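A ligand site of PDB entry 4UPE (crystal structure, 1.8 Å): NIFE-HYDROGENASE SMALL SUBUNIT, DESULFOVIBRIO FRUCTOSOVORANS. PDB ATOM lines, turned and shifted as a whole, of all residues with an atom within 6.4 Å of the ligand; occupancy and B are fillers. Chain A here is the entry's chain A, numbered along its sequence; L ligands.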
ATOM      1  N   VAL A 184      -1.303 -18.227  12.509  1.00  0.00           N
ATOM      2  CA  VAL A 184      -2.083 -18.071  13.710  1.00  0.00           C
ATOM      3  C   VAL A 184      -1.949 -19.334  14.547  1.00  0.00           C
ATOM      4  O   VAL A 184      -1.659 -19.270  15.734  1.00  0.00           O
ATOM      5  CB  VAL A 184      -3.580 -17.835  13.350  1.00  0.00           C
ATOM      6  CG1 VAL A 184      -4.501 -18.061  14.574  1.00  0.00           C
ATOM      7  CG2 VAL A 184      -3.788 -16.451  12.741  1.00  0.00           C
ATOM      8  N   HIS A 185      -2.099 -20.502  13.912  1.00  0.00           N
ATOM      9  CA  HIS A 185      -2.148 -21.791  14.593  1.00  0.00           C
ATOM     10  C   HIS A 185      -0.833 -22.055  15.335  1.00  0.00           C
ATOM     11  O   HIS A 185      -0.828 -22.664  16.396  1.00  0.00           O
ATOM     12  CB  HIS A 185      -2.395 -22.867  13.522  1.00  0.00           C
ATOM     13  CG  HIS A 185      -2.269 -24.297  13.975  1.00  0.00           C
ATOM     14  ND1 HIS A 185      -3.233 -24.945  14.723  1.00  0.00           N
ATOM     15  CD2 HIS A 185      -1.350 -25.232  13.655  1.00  0.00           C
ATOM     16  CE1 HIS A 185      -2.871 -26.203  14.901  1.00  0.00           C
ATOM     17  NE2 HIS A 185      -1.737 -26.404  14.259  1.00  0.00           N
ATOM     18  N   ASP A 186       0.281 -21.629  14.758  1.00  0.00           N
ATOM     19  CA  ASP A 186       1.588 -21.952  15.357  1.00  0.00           C
ATOM     20  C   ASP A 186       1.804 -21.251  16.722  1.00  0.00           C
ATOM     21  O   ASP A 186       2.627 -21.690  17.513  1.00  0.00           O
ATOM     22  CB  ASP A 186       2.741 -21.664  14.380  1.00  0.00           C
ATOM     23  CG  ASP A 186       2.854 -22.732  13.282  1.00  0.00           C
ATOM     24  OD1 ASP A 186       2.220 -23.801  13.380  1.00  0.00           O
ATOM     25  OD2 ASP A 186       3.572 -22.508  12.295  1.00  0.00           O
ATOM     26  N   CYS A 188      -0.963 -20.603  18.779  1.00  0.00           N
ATOM     27  CA  CYS A 188      -2.250 -20.726  19.466  1.00  0.00           C
ATOM     28  C   CYS A 188      -2.109 -21.486  20.797  1.00  0.00           C
ATOM     29  O   CYS A 188      -1.551 -22.563  20.817  1.00  0.00           O
ATOM     30  CB  CYS A 188      -3.260 -21.455  18.588  1.00  0.00           C
ATOM     31  SG  CYS A 188      -4.912 -21.516  19.314  1.00  0.00           S
ATOM     32  N   PRO A 189      -2.632 -20.921  21.897  1.00  0.00           N
ATOM     33  CA  PRO A 189      -2.581 -21.656  23.167  1.00  0.00           C
ATOM     34  C   PRO A 189      -3.326 -22.992  23.176  1.00  0.00           C
ATOM     35  O   PRO A 189      -3.123 -23.775  24.092  1.00  0.00           O
ATOM     36  CB  PRO A 189      -3.196 -20.681  24.190  1.00  0.00           C
ATOM     37  CG  PRO A 189      -2.945 -19.340  23.591  1.00  0.00           C
ATOM     38  CD  PRO A 189      -3.135 -19.550  22.097  1.00  0.00           C
ATOM     39  N   ARG A 190      -4.151 -23.256  22.170  1.00  0.00           N
ATOM     40  CA  ARG A 190      -4.867 -24.547  22.107  1.00  0.00           C
ATOM     41  C   ARG A 190      -4.093 -25.593  21.318  1.00  0.00           C
ATOM     42  O   ARG A 190      -4.555 -26.730  21.140  1.00  0.00           O
ATOM     43  CB  ARG A 190      -6.310 -24.378  21.570  1.00  0.00           C
ATOM     44  CG  ARG A 190      -7.123 -23.376  22.391  1.00  0.00           C
ATOM     45  CD  ARG A 190      -8.609 -23.407  22.065  1.00  0.00           C
ATOM     46  NE  ARG A 190      -9.276 -22.374  22.863  1.00  0.00           N
ATOM     47  CZ  ARG A 190     -10.564 -22.387  23.209  1.00  0.00           C
ATOM     48  NH1 ARG A 190     -11.353 -23.378  22.827  1.00  0.00           N
ATOM     49  NH2 ARG A 190     -11.065 -21.381  23.957  1.00  0.00           N
ATOM     50  N   LEU A 191      -2.908 -25.226  20.873  1.00  0.00           N
ATOM     51  CA  LEU A 191      -2.066 -26.136  20.087  1.00  0.00           C
ATOM     52  C   LEU A 191      -1.880 -27.517  20.698  1.00  0.00           C
ATOM     53  O   LEU A 191      -2.030 -28.522  19.982  1.00  0.00           O
ATOM     54  CB  LEU A 191      -0.707 -25.502  19.743  1.00  0.00           C
ATOM     55  CG  LEU A 191       0.159 -26.213  18.710  1.00  0.00           C
ATOM     56  CD1 LEU A 191      -0.595 -26.519  17.408  1.00  0.00           C
ATOM     57  CD2 LEU A 191       1.391 -25.352  18.431  1.00  0.00           C
ATOM     58  N   PRO A 192      -1.543 -27.603  22.014  1.00  0.00           N
ATOM     59  CA  PRO A 192      -1.449 -28.927  22.644  1.00  0.00           C
ATOM     60  C   PRO A 192      -2.709 -29.816  22.485  1.00  0.00           C
ATOM     61  O   PRO A 192      -2.566 -31.016  22.294  1.00  0.00           O
ATOM     62  CB  PRO A 192      -1.174 -28.622  24.131  1.00  0.00           C
ATOM     63  CG  PRO A 192      -0.641 -27.223  24.172  1.00  0.00           C
ATOM     64  CD  PRO A 192      -1.270 -26.506  22.984  1.00  0.00           C
ATOM     65  N   HIS A 193      -3.903 -29.223  22.536  1.00  0.00           N
ATOM     66  CA  HIS A 193      -5.138 -29.973  22.299  1.00  0.00           C
ATOM     67  C   HIS A 193      -5.186 -30.502  20.871  1.00  0.00           C
ATOM     68  O   HIS A 193      -5.506 -31.674  20.642  1.00  0.00           O
ATOM     69  CB  HIS A 193      -6.386 -29.131  22.638  1.00  0.00           C
ATOM     70  CG  HIS A 193      -6.566 -28.873  24.098  1.00  0.00           C
ATOM     71  ND1 HIS A 193      -6.699 -29.883  25.034  1.00  0.00           N
ATOM     72  CD2 HIS A 193      -6.634 -27.706  24.791  1.00  0.00           C
ATOM     73  CE1 HIS A 193      -6.848 -29.352  26.240  1.00  0.00           C
ATOM     74  NE2 HIS A 193      -6.815 -28.039  26.126  1.00  0.00           N
ATOM     75  N   PHE A 194      -4.849 -29.644  19.910  1.00  0.00           N
ATOM     76  CA  PHE A 194      -4.813 -30.025  18.515  1.00  0.00           C
ATOM     77  C   PHE A 194      -3.822 -31.198  18.346  1.00  0.00           C
ATOM     78  O   PHE A 194      -4.145 -32.212  17.708  1.00  0.00           O
ATOM     79  CB  PHE A 194      -4.424 -28.820  17.639  1.00  0.00           C
ATOM     80  CG  PHE A 194      -4.235 -29.155  16.152  1.00  0.00           C
ATOM     81  CD1 PHE A 194      -3.002 -29.641  15.667  1.00  0.00           C
ATOM     82  CD2 PHE A 194      -5.278 -28.942  15.238  1.00  0.00           C
ATOM     83  CE1 PHE A 194      -2.832 -29.897  14.295  1.00  0.00           C
ATOM     84  CE2 PHE A 194      -5.112 -29.196  13.858  1.00  0.00           C
ATOM     85  CZ  PHE A 194      -3.875 -29.684  13.382  1.00  0.00           C
ATOM     86  N   PHE A 199     -10.564 -32.274  20.352  1.00  0.00           N
ATOM     87  CA  PHE A 199     -11.348 -31.282  19.608  1.00  0.00           C
ATOM     88  C   PHE A 199     -12.738 -31.163  20.234  1.00  0.00           C
ATOM     89  O   PHE A 199     -13.353 -32.174  20.562  1.00  0.00           O
ATOM     90  CB  PHE A 199     -11.509 -31.717  18.139  1.00  0.00           C
ATOM     91  CG  PHE A 199     -10.205 -31.979  17.412  1.00  0.00           C
ATOM     92  CD1 PHE A 199      -9.310 -30.939  17.142  1.00  0.00           C
ATOM     93  CD2 PHE A 199      -9.874 -33.275  16.974  1.00  0.00           C
ATOM     94  CE1 PHE A 199      -8.117 -31.174  16.482  1.00  0.00           C
ATOM     95  CE2 PHE A 199      -8.673 -33.524  16.329  1.00  0.00           C
ATOM     96  CZ  PHE A 199      -7.804 -32.471  16.054  1.00  0.00           C
ATOM     97  N   PHE A 212     -10.942 -26.912  24.505  1.00  0.00           N
ATOM     98  CA  PHE A 212     -10.375 -27.834  23.499  1.00  0.00           C
ATOM     99  C   PHE A 212     -10.241 -27.111  22.151  1.00  0.00           C
ATOM    100  O   PHE A 212     -10.890 -26.056  21.916  1.00  0.00           O
ATOM    101  CB  PHE A 212     -11.248 -29.089  23.355  1.00  0.00           C
ATOM    102  CG  PHE A 212     -10.965 -30.192  24.369  1.00  0.00           C
ATOM    103  CD1 PHE A 212     -10.492 -29.903  25.653  1.00  0.00           C
ATOM    104  CD2 PHE A 212     -11.236 -31.525  24.056  1.00  0.00           C
ATOM    105  CE1 PHE A 212     -10.249 -30.918  26.573  1.00  0.00           C
ATOM    106  CE2 PHE A 212     -11.014 -32.529  24.980  1.00  0.00           C
ATOM    107  CZ  PHE A 212     -10.510 -32.236  26.236  1.00  0.00           C
ATOM    108  N   CYS A 213      -9.385 -27.671  21.273  1.00  0.00           N
ATOM    109  CA  CYS A 213      -9.124 -27.121  19.946  1.00  0.00           C
ATOM    110  C   CYS A 213     -10.417 -26.982  19.156  1.00  0.00           C
ATOM    111  O   CYS A 213     -11.346 -27.819  19.281  1.00  0.00           O
ATOM    112  CB  CYS A 213      -8.073 -27.979  19.193  1.00  0.00           C
ATOM    113  SG  CYS A 213      -7.816 -27.539  17.450  1.00  0.00           S
ATOM    114  N   LEU A 214     -10.480 -25.954  18.319  1.00  0.00           N
ATOM    115  CA  LEU A 214     -11.698 -25.652  17.548  1.00  0.00           C
ATOM    116  C   LEU A 214     -11.616 -26.080  16.068  1.00  0.00           C
ATOM    117  O   LEU A 214     -12.374 -25.606  15.230  1.00  0.00           O
ATOM    118  CB  LEU A 214     -12.047 -24.158  17.678  1.00  0.00           C
ATOM    119  CG  LEU A 214     -12.119 -23.618  19.115  1.00  0.00           C
ATOM    120  CD1 LEU A 214     -12.169 -22.092  19.106  1.00  0.00           C
ATOM    121  CD2 LEU A 214     -13.282 -24.250  19.893  1.00  0.00           C
ATOM    122  N   TYR A 215     -10.663 -26.961  15.770  1.00  0.00           N
ATOM    123  CA  TYR A 215     -10.433 -27.380  14.401  1.00  0.00           C
ATOM    124  C   TYR A 215     -11.670 -28.050  13.778  1.00  0.00           C
ATOM    125  O   TYR A 215     -12.029 -27.782  12.620  1.00  0.00           O
ATOM    126  CB  TYR A 215      -9.198 -28.314  14.334  1.00  0.00           C
ATOM    127  CG  TYR A 215      -8.731 -28.604  12.922  1.00  0.00           C
ATOM    128  CD1 TYR A 215      -8.269 -27.584  12.094  1.00  0.00           C
ATOM    129  CD2 TYR A 215      -8.750 -29.911  12.423  1.00  0.00           C
ATOM    130  CE1 TYR A 215      -7.842 -27.866  10.800  1.00  0.00           C
ATOM    131  CE2 TYR A 215      -8.332 -30.193  11.134  1.00  0.00           C
ATOM    132  CZ  TYR A 215      -7.900 -29.166  10.335  1.00  0.00           C
ATOM    133  OH  TYR A 215      -7.440 -29.445   9.059  1.00  0.00           O
ATOM    134  N   CYS A 219     -11.994 -24.115  12.510  1.00  0.00           N
ATOM    135  CA  CYS A 219     -10.920 -23.132  12.749  1.00  0.00           C
ATOM    136  C   CYS A 219      -9.913 -23.158  11.594  1.00  0.00           C
ATOM    137  O   CYS A 219      -9.407 -24.219  11.259  1.00  0.00           O
ATOM    138  CB  CYS A 219     -10.138 -23.446  14.042  1.00  0.00           C
ATOM    139  SG  CYS A 219      -9.029 -22.054  14.463  1.00  0.00           S
ATOM    140  N   LYS A 220      -9.648 -21.994  10.995  1.00  0.00           N
ATOM    141  CA  LYS A 220      -8.740 -21.878   9.851  1.00  0.00           C
ATOM    142  C   LYS A 220      -7.351 -21.377  10.285  1.00  0.00           C
ATOM    143  O   LYS A 220      -6.503 -21.003   9.483  1.00  0.00           O
ATOM    144  CB  LYS A 220      -9.384 -20.988   8.769  1.00  0.00           C
ATOM    145  CG  LYS A 220     -10.758 -21.518   8.320  1.00  0.00           C
ATOM    146  CD  LYS A 220     -10.737 -22.995   7.913  1.00  0.00           C
ATOM    147  CE  LYS A 220     -12.018 -23.427   7.173  1.00  0.00           C
ATOM    148  NZ  LYS A 220     -13.282 -23.024   7.896  1.00  0.00           N
ATOM    149  N   GLY A 221      -7.104 -21.375  11.582  1.00  0.00           N
ATOM    150  CA  GLY A 221      -5.794 -20.957  12.056  1.00  0.00           C
ATOM    151  C   GLY A 221      -4.630 -21.704  11.392  1.00  0.00           C
ATOM    152  O   GLY A 221      -3.597 -21.066  11.095  1.00  0.00           O
ATOM    153  N   PRO A 222      -4.782 -23.026  11.111  1.00  0.00           N
ATOM    154  CA  PRO A 222      -3.658 -23.729  10.457  1.00  0.00           C
ATOM    155  C   PRO A 222      -3.276 -23.248   9.058  1.00  0.00           C
ATOM    156  O   PRO A 222      -2.214 -23.607   8.596  1.00  0.00           O
ATOM    157  CB  PRO A 222      -4.141 -25.197  10.381  1.00  0.00           C
ATOM    158  CG  PRO A 222      -5.178 -25.314  11.453  1.00  0.00           C
ATOM    159  CD  PRO A 222      -5.857 -23.973  11.469  1.00  0.00           C
ATOM    160  N   TRP A 238      -8.622 -12.264  21.711  1.00  0.00           N
ATOM    161  CA  TRP A 238      -8.642 -12.655  20.297  1.00  0.00           C
ATOM    162  C   TRP A 238      -9.700 -13.751  20.087  1.00  0.00           C
ATOM    163  O   TRP A 238     -10.127 -14.370  21.036  1.00  0.00           O
ATOM    164  CB  TRP A 238      -7.243 -13.035  19.765  1.00  0.00           C
ATOM    165  CG  TRP A 238      -6.668 -14.359  20.172  1.00  0.00           C
ATOM    166  CD1 TRP A 238      -6.212 -14.717  21.405  1.00  0.00           C
ATOM    167  CD2 TRP A 238      -6.431 -15.484  19.308  1.00  0.00           C
ATOM    168  NE1 TRP A 238      -5.722 -16.012  21.374  1.00  0.00           N
ATOM    169  CE2 TRP A 238      -5.832 -16.495  20.087  1.00  0.00           C
ATOM    170  CE3 TRP A 238      -6.655 -15.730  17.939  1.00  0.00           C
ATOM    171  CZ2 TRP A 238      -5.479 -17.749  19.544  1.00  0.00           C
ATOM    172  CZ3 TRP A 238      -6.301 -16.974  17.399  1.00  0.00           C
ATOM    173  CH2 TRP A 238      -5.712 -17.964  18.224  1.00  0.00           C
ATOM    174  N   VAL A 240     -10.122 -16.958  19.202  1.00  0.00           N
ATOM    175  CA  VAL A 240      -9.983 -18.307  19.789  1.00  0.00           C
ATOM    176  C   VAL A 240      -9.992 -18.253  21.331  1.00  0.00           C
ATOM    177  O   VAL A 240     -10.606 -19.098  21.964  1.00  0.00           O
ATOM    178  CB  VAL A 240      -8.745 -19.079  19.241  1.00  0.00           C
ATOM    179  CG1 VAL A 240      -8.382 -20.275  20.127  1.00  0.00           C
ATOM    180  CG2 VAL A 240      -8.952 -19.524  17.794  1.00  0.00           C
ATOM    181  N   PRO A 245     -13.723 -20.208  16.400  1.00  0.00           N
ATOM    182  CA  PRO A 245     -12.717 -20.500  15.367  1.00  0.00           C
ATOM    183  C   PRO A 245     -12.271 -19.260  14.576  1.00  0.00           C
ATOM    184  O   PRO A 245     -13.014 -18.301  14.398  1.00  0.00           O
ATOM    185  CB  PRO A 245     -13.428 -21.509  14.446  1.00  0.00           C
ATOM    186  CG  PRO A 245     -14.918 -21.368  14.758  1.00  0.00           C
ATOM    187  CD  PRO A 245     -14.973 -20.990  16.221  1.00  0.00           C
ATOM    188  N   CYS A 246     -11.012 -19.278  14.155  1.00  0.00           N
ATOM    189  CA  CYS A 246     -10.495 -18.330  13.171  1.00  0.00           C
ATOM    190  C   CYS A 246     -11.204 -18.468  11.789  1.00  0.00           C
ATOM    191  O   CYS A 246     -11.453 -19.589  11.267  1.00  0.00           O
ATOM    192  CB  CYS A 246      -8.981 -18.560  13.008  1.00  0.00           C
ATOM    193  SG  CYS A 246      -8.202 -17.496  11.754  1.00  0.00           S
ATOM    194  N   GLN A 264     -14.492 -27.939   7.932  1.00  0.00           N
ATOM    195  CA  GLN A 264     -13.184 -28.044   7.236  1.00  0.00           C
ATOM    196  C   GLN A 264     -13.352 -28.603   5.817  1.00  0.00           C
ATOM    197  O   GLN A 264     -12.377 -29.012   5.211  1.00  0.00           O
ATOM    198  CB  GLN A 264     -12.198 -28.908   8.003  1.00  0.00           C
ATOM    199  CG  GLN A 264     -11.734 -28.377   9.361  1.00  0.00           C
ATOM    200  CD  GLN A 264     -10.874 -27.100   9.332  1.00  0.00           C
ATOM    201  OE1 GLN A 264     -10.363 -26.674   8.281  1.00  0.00           O
ATOM    202  NE2 GLN A 264     -10.719 -26.480  10.495  1.00  0.00           N
HETATM  203 FE1  LIG L   1      -6.922 -25.453  17.252  1.00  0.00          FE
HETATM  204 FE2  LIG L   1      -5.836 -23.021  17.871  1.00  0.00          FE
HETATM  205 FE3  LIG L   1      -5.039 -24.297  15.668  1.00  0.00          FE
HETATM  206 FE4  LIG L   1      -7.474 -23.152  15.700  1.00  0.00          FE
HETATM  207  S1  LIG L   1      -5.479 -22.018  15.841  1.00  0.00           S
HETATM  208  S2  LIG L   1      -7.015 -25.195  14.906  1.00  0.00           S
HETATM  209  S3  LIG L   1      -8.063 -23.591  17.948  1.00  0.00           S
HETATM  210  S4  LIG L   1      -4.790 -25.085  17.822  1.00  0.00           S
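The backbone NH (N) of Leu 214 sits close to a sulfur (S3) of the ligand (3.4 Å).
SG of Cys 188 is bound to FE2 of the ligand, at 2.3 Å.
FE1 of the ligand is bound by SG of Cys 213, 2.3 Å away.
A sulfur (S4) of the ligand lies close to the backbone NH of Leu 191, at 3.6 Å.
SG of Cys 219 binds FE4 of the ligand (2.3 Å).
An iron atom (FE3) of the ligand is bound by a ring nitrogen (ND1) of His 185 (2.1 Å).
O of Cys 219 is in hydrogen-bond range of NE2 of Gln 264 (2.7 Å).
The side-chain sulfur (SG) of Cys 219 sits close to the backbone NH (N) of Gly 221, at 3.5 Å.
The backbone NH of Tyr 215 lies close to the side-chain sulfur of Cys 213 (3.4 Å).
The backbone carbonyl oxygen (O) of Phe 212 is in hydrogen-bond range of the guanidinium group (NH1) of Arg 190 (2.9 Å).
O of Val 240 sits at hydrogen-bond distance from NH2 of Arg 190.
The backbone NH of His 185 sits at hydrogen-bond distance from the backbone carbonyl oxygen of Gly 221 (3.2 Å).
The side-chain sulfur of Cys 219 sits close to the backbone NH of Cys 246 (3.4 Å).
N of Arg 190 lies close to SG of Cys 188 (3.4 Å).
O of Arg 190 lies close to S4 of the ligand (3.7 Å).
Residues that only touch the ligand: Phe 194 (3.8 Å), Pro 222 (3.8 Å), Tyr 215 (3.8 Å), Gly 221 (3.9 Å) and Val 240 (3.98 Å).
Hydrophobic or aromatic side chains that line the ligand: His 185, Phe 194, Tyr 215, Pro 222 and Val 240.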
